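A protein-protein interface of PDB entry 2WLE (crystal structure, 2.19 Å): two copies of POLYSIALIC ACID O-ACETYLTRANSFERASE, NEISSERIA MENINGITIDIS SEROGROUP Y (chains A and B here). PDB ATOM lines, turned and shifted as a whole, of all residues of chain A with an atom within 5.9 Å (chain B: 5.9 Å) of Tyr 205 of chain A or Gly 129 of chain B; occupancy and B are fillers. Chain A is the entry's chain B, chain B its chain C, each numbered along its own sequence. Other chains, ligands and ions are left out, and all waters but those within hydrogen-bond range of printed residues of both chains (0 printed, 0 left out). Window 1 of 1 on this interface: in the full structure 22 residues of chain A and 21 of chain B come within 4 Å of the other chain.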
ATOM      1  N   SER A 202       8.929  21.263  11.720  1.00  0.00           N
ATOM      2  CA  SER A 202       9.350  21.626  13.068  1.00  0.00           C
ATOM      3  C   SER A 202       8.700  22.928  13.530  1.00  0.00           C
ATOM      4  O   SER A 202       8.307  23.061  14.689  1.00  0.00           O
ATOM      5  CB  SER A 202      10.876  21.734  13.143  1.00  0.00           C
ATOM      6  OG  SER A 202      11.430  22.030  11.876  1.00  0.00           O
ATOM      7  N   THR A 203       8.594  23.892  12.624  1.00  0.00           N
ATOM      8  CA  THR A 203       7.963  25.161  12.949  1.00  0.00           C
ATOM      9  C   THR A 203       6.907  25.476  11.914  1.00  0.00           C
ATOM     10  O   THR A 203       6.905  24.908  10.822  1.00  0.00           O
ATOM     11  CB  THR A 203       8.978  26.329  12.947  1.00  0.00           C
ATOM     12  OG1 THR A 203       9.392  26.596  11.604  1.00  0.00           O
ATOM     13  CG2 THR A 203      10.184  25.996  13.799  1.00  0.00           C
ATOM     14  N   MET A 204       6.021  26.401  12.251  1.00  0.00           N
ATOM     15  CA  MET A 204       4.981  26.801  11.326  1.00  0.00           C
ATOM     16  C   MET A 204       5.581  27.383  10.052  1.00  0.00           C
ATOM     17  O   MET A 204       4.947  27.349   8.999  1.00  0.00           O
ATOM     18  CB  MET A 204       4.030  27.804  11.981  1.00  0.00           C
ATOM     19  CG  MET A 204       4.605  29.179  12.223  1.00  0.00           C
ATOM     20  SD  MET A 204       3.438  30.205  13.129  1.00  0.00           S
ATOM     21  CE  MET A 204       4.284  31.783  13.179  1.00  0.00           C
ATOM     22  N   TYR A 205       6.806  27.901  10.147  1.00  0.00           N
ATOM     23  CA  TYR A 205       7.465  28.532   9.010  1.00  0.00           C
ATOM     24  C   TYR A 205       7.862  27.519   7.941  1.00  0.00           C
ATOM     25  O   TYR A 205       8.066  27.879   6.784  1.00  0.00           O
ATOM     26  CB  TYR A 205       8.694  29.320   9.480  1.00  0.00           C
ATOM     27  CG  TYR A 205       8.352  30.366  10.515  1.00  0.00           C
ATOM     28  CD1 TYR A 205       8.782  30.250  11.830  1.00  0.00           C
ATOM     29  CD2 TYR A 205       7.570  31.456  10.180  1.00  0.00           C
ATOM     30  CE1 TYR A 205       8.451  31.204  12.772  1.00  0.00           C
ATOM     31  CE2 TYR A 205       7.237  32.409  11.111  1.00  0.00           C
ATOM     32  CZ  TYR A 205       7.676  32.283  12.401  1.00  0.00           C
ATOM     33  OH  TYR A 205       7.330  33.246  13.314  1.00  0.00           O
ATOM     34  N   ASP A 206       7.967  26.255   8.333  1.00  0.00           N
ATOM     35  CA  ASP A 206       8.308  25.193   7.397  1.00  0.00           C
ATOM     36  C   ASP A 206       7.063  24.689   6.676  1.00  0.00           C
ATOM     37  O   ASP A 206       7.141  23.748   5.890  1.00  0.00           O
ATOM     38  CB  ASP A 206       8.973  24.028   8.130  1.00  0.00           C
ATOM     39  CG  ASP A 206      10.181  24.458   8.939  1.00  0.00           C
ATOM     40  OD1 ASP A 206      11.192  24.857   8.333  1.00  0.00           O
ATOM     41  OD2 ASP A 206      10.124  24.381  10.184  1.00  0.00           O
ATOM     42  N   ASP A 207       5.917  25.311   6.943  1.00  0.00           N
ATOM     43  CA  ASP A 207       4.662  24.893   6.320  1.00  0.00           C
ATOM     44  C   ASP A 207       4.090  25.996   5.440  1.00  0.00           C
ATOM     45  O   ASP A 207       3.571  26.990   5.943  1.00  0.00           O
ATOM     46  CB  ASP A 207       3.638  24.499   7.388  1.00  0.00           C
ATOM     47  CG  ASP A 207       2.401  23.842   6.797  1.00  0.00           C
ATOM     48  OD1 ASP A 207       2.415  23.495   5.595  1.00  0.00           O
ATOM     49  OD2 ASP A 207       1.415  23.676   7.534  1.00  0.00           O
ATOM     50  N   PRO A 208       4.163  25.811   4.113  1.00  0.00           N
ATOM     51  CA  PRO A 208       3.732  26.850   3.186  1.00  0.00           C
ATOM     52  C   PRO A 208       2.241  27.136   3.306  1.00  0.00           C
ATOM     53  O   PRO A 208       1.794  28.242   3.010  1.00  0.00           O
ATOM     54  CB  PRO A 208       4.060  26.268   1.801  1.00  0.00           C
ATOM     55  CG  PRO A 208       4.759  24.965   2.037  1.00  0.00           C
ATOM     56  CD  PRO A 208       4.487  24.548   3.433  1.00  0.00           C
ATOM     57  N   ASN A 211       1.364  30.136   5.897  1.00  0.00           N
ATOM     58  CA  ASN A 211       1.831  31.508   5.728  1.00  0.00           C
ATOM     59  C   ASN A 211       0.765  32.537   6.105  1.00  0.00           C
ATOM     60  O   ASN A 211       1.053  33.521   6.783  1.00  0.00           O
ATOM     61  CB  ASN A 211       2.292  31.739   4.283  1.00  0.00           C
ATOM     62  CG  ASN A 211       3.511  30.907   3.915  1.00  0.00           C
ATOM     63  OD1 ASN A 211       4.062  31.047   2.830  1.00  0.00           O
ATOM     64  ND2 ASN A 211       3.933  30.036   4.821  1.00  0.00           N
ATOM     65  N   TYR A 214      -0.004  33.586   9.979  1.00  0.00           N
ATOM     66  CA  TYR A 214       0.931  34.419  10.722  1.00  0.00           C
ATOM     67  C   TYR A 214       1.421  35.566   9.852  1.00  0.00           C
ATOM     68  O   TYR A 214       1.168  36.731  10.149  1.00  0.00           O
ATOM     69  CB  TYR A 214       2.116  33.588  11.207  1.00  0.00           C
ATOM     70  CG  TYR A 214       2.986  33.060  10.090  1.00  0.00           C
ATOM     71  CD1 TYR A 214       3.841  33.900   9.392  1.00  0.00           C
ATOM     72  CD2 TYR A 214       2.954  31.720   9.735  1.00  0.00           C
ATOM     73  CE1 TYR A 214       4.639  33.421   8.373  1.00  0.00           C
ATOM     74  CE2 TYR A 214       3.749  31.232   8.716  1.00  0.00           C
ATOM     75  CZ  TYR A 214       4.588  32.086   8.041  1.00  0.00           C
ATOM     76  OH  TYR A 214       5.383  31.606   7.027  1.00  0.00           O
ATOM     77  N   TYR B 124       1.172  24.865  16.635  1.00  0.00           N
ATOM     78  CA  TYR B 124       2.256  25.828  16.775  1.00  0.00           C
ATOM     79  C   TYR B 124       1.799  27.077  17.518  1.00  0.00           C
ATOM     80  O   TYR B 124       0.659  27.523  17.361  1.00  0.00           O
ATOM     81  CB  TYR B 124       2.782  26.256  15.403  1.00  0.00           C
ATOM     82  CG  TYR B 124       3.154  25.133  14.463  1.00  0.00           C
ATOM     83  CD1 TYR B 124       4.356  24.460  14.588  1.00  0.00           C
ATOM     84  CD2 TYR B 124       2.306  24.767  13.427  1.00  0.00           C
ATOM     85  CE1 TYR B 124       4.702  23.447  13.712  1.00  0.00           C
ATOM     86  CE2 TYR B 124       2.642  23.755  12.544  1.00  0.00           C
ATOM     87  CZ  TYR B 124       3.838  23.103  12.687  1.00  0.00           C
ATOM     88  OH  TYR B 124       4.162  22.096  11.806  1.00  0.00           O
ATOM     89  N   SER B 125       2.706  27.647  18.307  1.00  0.00           N
ATOM     90  CA  SER B 125       2.468  28.941  18.940  1.00  0.00           C
ATOM     91  C   SER B 125       2.568  30.068  17.914  1.00  0.00           C
ATOM     92  O   SER B 125       3.484  30.091  17.096  1.00  0.00           O
ATOM     93  CB  SER B 125       3.491  29.192  20.056  1.00  0.00           C
ATOM     94  OG  SER B 125       3.514  30.563  20.415  1.00  0.00           O
ATOM     95  N   LEU B 126       1.623  31.003  17.967  1.00  0.00           N
ATOM     96  CA  LEU B 126       1.675  32.198  17.127  1.00  0.00           C
ATOM     97  C   LEU B 126       2.769  33.161  17.595  1.00  0.00           C
ATOM     98  O   LEU B 126       3.289  33.956  16.815  1.00  0.00           O
ATOM     99  CB  LEU B 126       0.317  32.905  17.126  1.00  0.00           C
ATOM    100  CG  LEU B 126      -0.444  32.844  15.794  1.00  0.00           C
ATOM    101  CD1 LEU B 126       0.012  31.647  14.972  1.00  0.00           C
ATOM    102  CD2 LEU B 126      -1.952  32.832  16.010  1.00  0.00           C
ATOM    103  N   GLU B 127       3.124  33.075  18.874  1.00  0.00           N
ATOM    104  CA  GLU B 127       4.131  33.966  19.444  1.00  0.00           C
ATOM    105  C   GLU B 127       5.508  33.750  18.807  1.00  0.00           C
ATOM    106  O   GLU B 127       6.177  34.712  18.426  1.00  0.00           O
ATOM    107  CB  GLU B 127       4.190  33.790  20.970  1.00  0.00           C
ATOM    108  CG  GLU B 127       2.871  34.143  21.678  1.00  0.00           C
ATOM    109  CD  GLU B 127       2.932  34.000  23.193  1.00  0.00           C
ATOM    110  OE1 GLU B 127       3.896  34.500  23.815  1.00  0.00           O
ATOM    111  OE2 GLU B 127       1.999  33.391  23.763  1.00  0.00           O
ATOM    112  N   ASN B 128       5.928  32.495  18.672  1.00  0.00           N
ATOM    113  CA  ASN B 128       7.287  32.203  18.199  1.00  0.00           C
ATOM    114  C   ASN B 128       7.363  31.067  17.165  1.00  0.00           C
ATOM    115  O   ASN B 128       8.450  30.617  16.804  1.00  0.00           O
ATOM    116  CB  ASN B 128       8.191  31.882  19.393  1.00  0.00           C
ATOM    117  CG  ASN B 128       7.747  30.652  20.136  1.00  0.00           C
ATOM    118  OD1 ASN B 128       6.927  29.880  19.640  1.00  0.00           O
ATOM    119  ND2 ASN B 128       8.283  30.456  21.336  1.00  0.00           N
ATOM    120  N   GLY B 129       6.213  30.601  16.691  1.00  0.00           N
ATOM    121  CA  GLY B 129       6.177  29.590  15.629  1.00  0.00           C
ATOM    122  C   GLY B 129       6.548  28.178  16.062  1.00  0.00           C
ATOM    123  O   GLY B 129       6.551  27.240  15.246  1.00  0.00           O
ATOM    124  N   GLU B 130       6.850  28.013  17.346  1.00  0.00           N
ATOM    125  CA  GLU B 130       7.343  26.738  17.847  1.00  0.00           C
ATOM    126  C   GLU B 130       6.204  25.750  18.062  1.00  0.00           C
ATOM    127  O   GLU B 130       5.062  26.149  18.302  1.00  0.00           O
ATOM    128  CB  GLU B 130       8.123  26.937  19.149  1.00  0.00           C
ATOM    129  CG  GLU B 130       9.366  27.796  18.982  1.00  0.00           C
ATOM    130  CD  GLU B 130      10.112  27.490  17.689  1.00  0.00           C
ATOM    131  OE1 GLU B 130      10.491  26.320  17.468  1.00  0.00           O
ATOM    132  OE2 GLU B 130      10.321  28.423  16.885  1.00  0.00           O
ATOM    133  N   ARG B 131       6.520  24.462  17.969  1.00  0.00           N
ATOM    134  CA  ARG B 131       5.551  23.407  18.276  1.00  0.00           C
ATOM    135  C   ARG B 131       5.383  23.262  19.785  1.00  0.00           C
ATOM    136  O   ARG B 131       6.366  23.202  20.513  1.00  0.00           O
ATOM    137  CB  ARG B 131       5.984  22.066  17.686  1.00  0.00           C
ATOM    138  CG  ARG B 131       4.916  21.010  17.884  1.00  0.00           C
ATOM    139  CD  ARG B 131       5.248  19.631  17.327  1.00  0.00           C
ATOM    140  NE  ARG B 131       4.154  18.712  17.658  1.00  0.00           N
ATOM    141  CZ  ARG B 131       4.138  17.412  17.392  1.00  0.00           C
ATOM    142  NH1 ARG B 131       5.156  16.830  16.778  1.00  0.00           N
ATOM    143  NH2 ARG B 131       3.083  16.694  17.741  1.00  0.00           N
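N of Met 204 of chain A sits at hydrogen-bond distance from O of Gly 129 of chain B (3.2 Å).
OG of Ser 202 of chain A sits at hydrogen-bond distance from OD2 of Asp 206 of chain A (3.2 Å). The side-chain hydroxyl (OG1) of Thr 203 of chain A lies within hydrogen-bond range of the side-chain carboxylate (OD2) of Asp 206 of chain A (2.7 Å). OD1 of Asn 128 of chain B is in hydrogen-bond range of N of Glu 130 of chain B (3.0 Å). The backbone carbonyl oxygen (O) of Glu 130 of chain B sits at hydrogen-bond distance from the backbone NH (N) of Ser 125 of chain B, 2.8 Å away. The side-chain hydroxyl (OG) of Ser 125 of chain B lies within hydrogen-bond range of the backbone NH (N) of Glu 127 of chain B, at 3.0 Å. The backbone NH of Tyr 205 of chain A sits close to the side-chain hydroxyl of Thr 203 of chain A.
Among the printed residues, pairs that only touch across the chains: Ser 202 of chain A with Tyr 124 of chain B (3.8 Å), Ser 202 of chain A with Arg 131 of chain B (3.9 Å), Thr 203 of chain A with Tyr 124 of chain B (3.5 Å), Thr 203 of chain A with Gly 129 of chain B (3.4 Å), Thr 203 of chain A with Glu 130 of chain B (3.7 Å), Met 204 of chain A with Tyr 124 of chain B (3.5 Å), Met 204 of chain A with Ser 125 of chain B (3.97 Å) and Tyr 205 of chain A with Gly 129 of chain B (3.99 Å).
Printed residues of chain B within 4 Å of Ser 202 of chain A: Tyr 124 (3.8 Å) and Arg 131 (3.9 Å). Of the printed residues of chain B, Tyr 205 of chain A touches Gly 129 (3.99 Å). Of the printed residues of chain A, Tyr 124 of chain B touches Ser 202 (3.8 Å), Thr 203 (3.5 Å) and Met 204 (3.5 Å). Printed residues of chain A within 4 Å of Ser 125 of chain B: Met 204 (3.97 Å). Leu 126 of chain B touches none of the printed residues of chain A. Asn 128 of chain B touches none of the printed residues of chain A. Printed residues of chain A within 4 Å of Gly 129 of chain B: Thr 203 (3.4 Å), Met 204 (3.2 Å) and Tyr 205 (3.99 Å). Printed residues of chain A within 4 Å of Glu 130 of chain B: Thr 203. Printed residues of chain A within 4 Å of Arg 131 of chain B: Ser 202. The nearest printed residue of chain B that does not touch Tyr 205 of chain A is Asn 128 of chain B (4.1 Å). The nearest printed residue of chain A that does not touch Gly 129 of chain B is Ser 202 of chain A (4.6 Å).
Hydrophobic or aromatic side chains of chain A within 4 Å of the printed part of chain B: Met 204 and Tyr 205. Hydrophobic or aromatic side chains of chain B that line the printed part of chain A: Tyr 124.
No position is printed for both chains. Of the 9 pairs that touch across the chains among the printed residues, none has its exchanged pair printed and touching as well.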
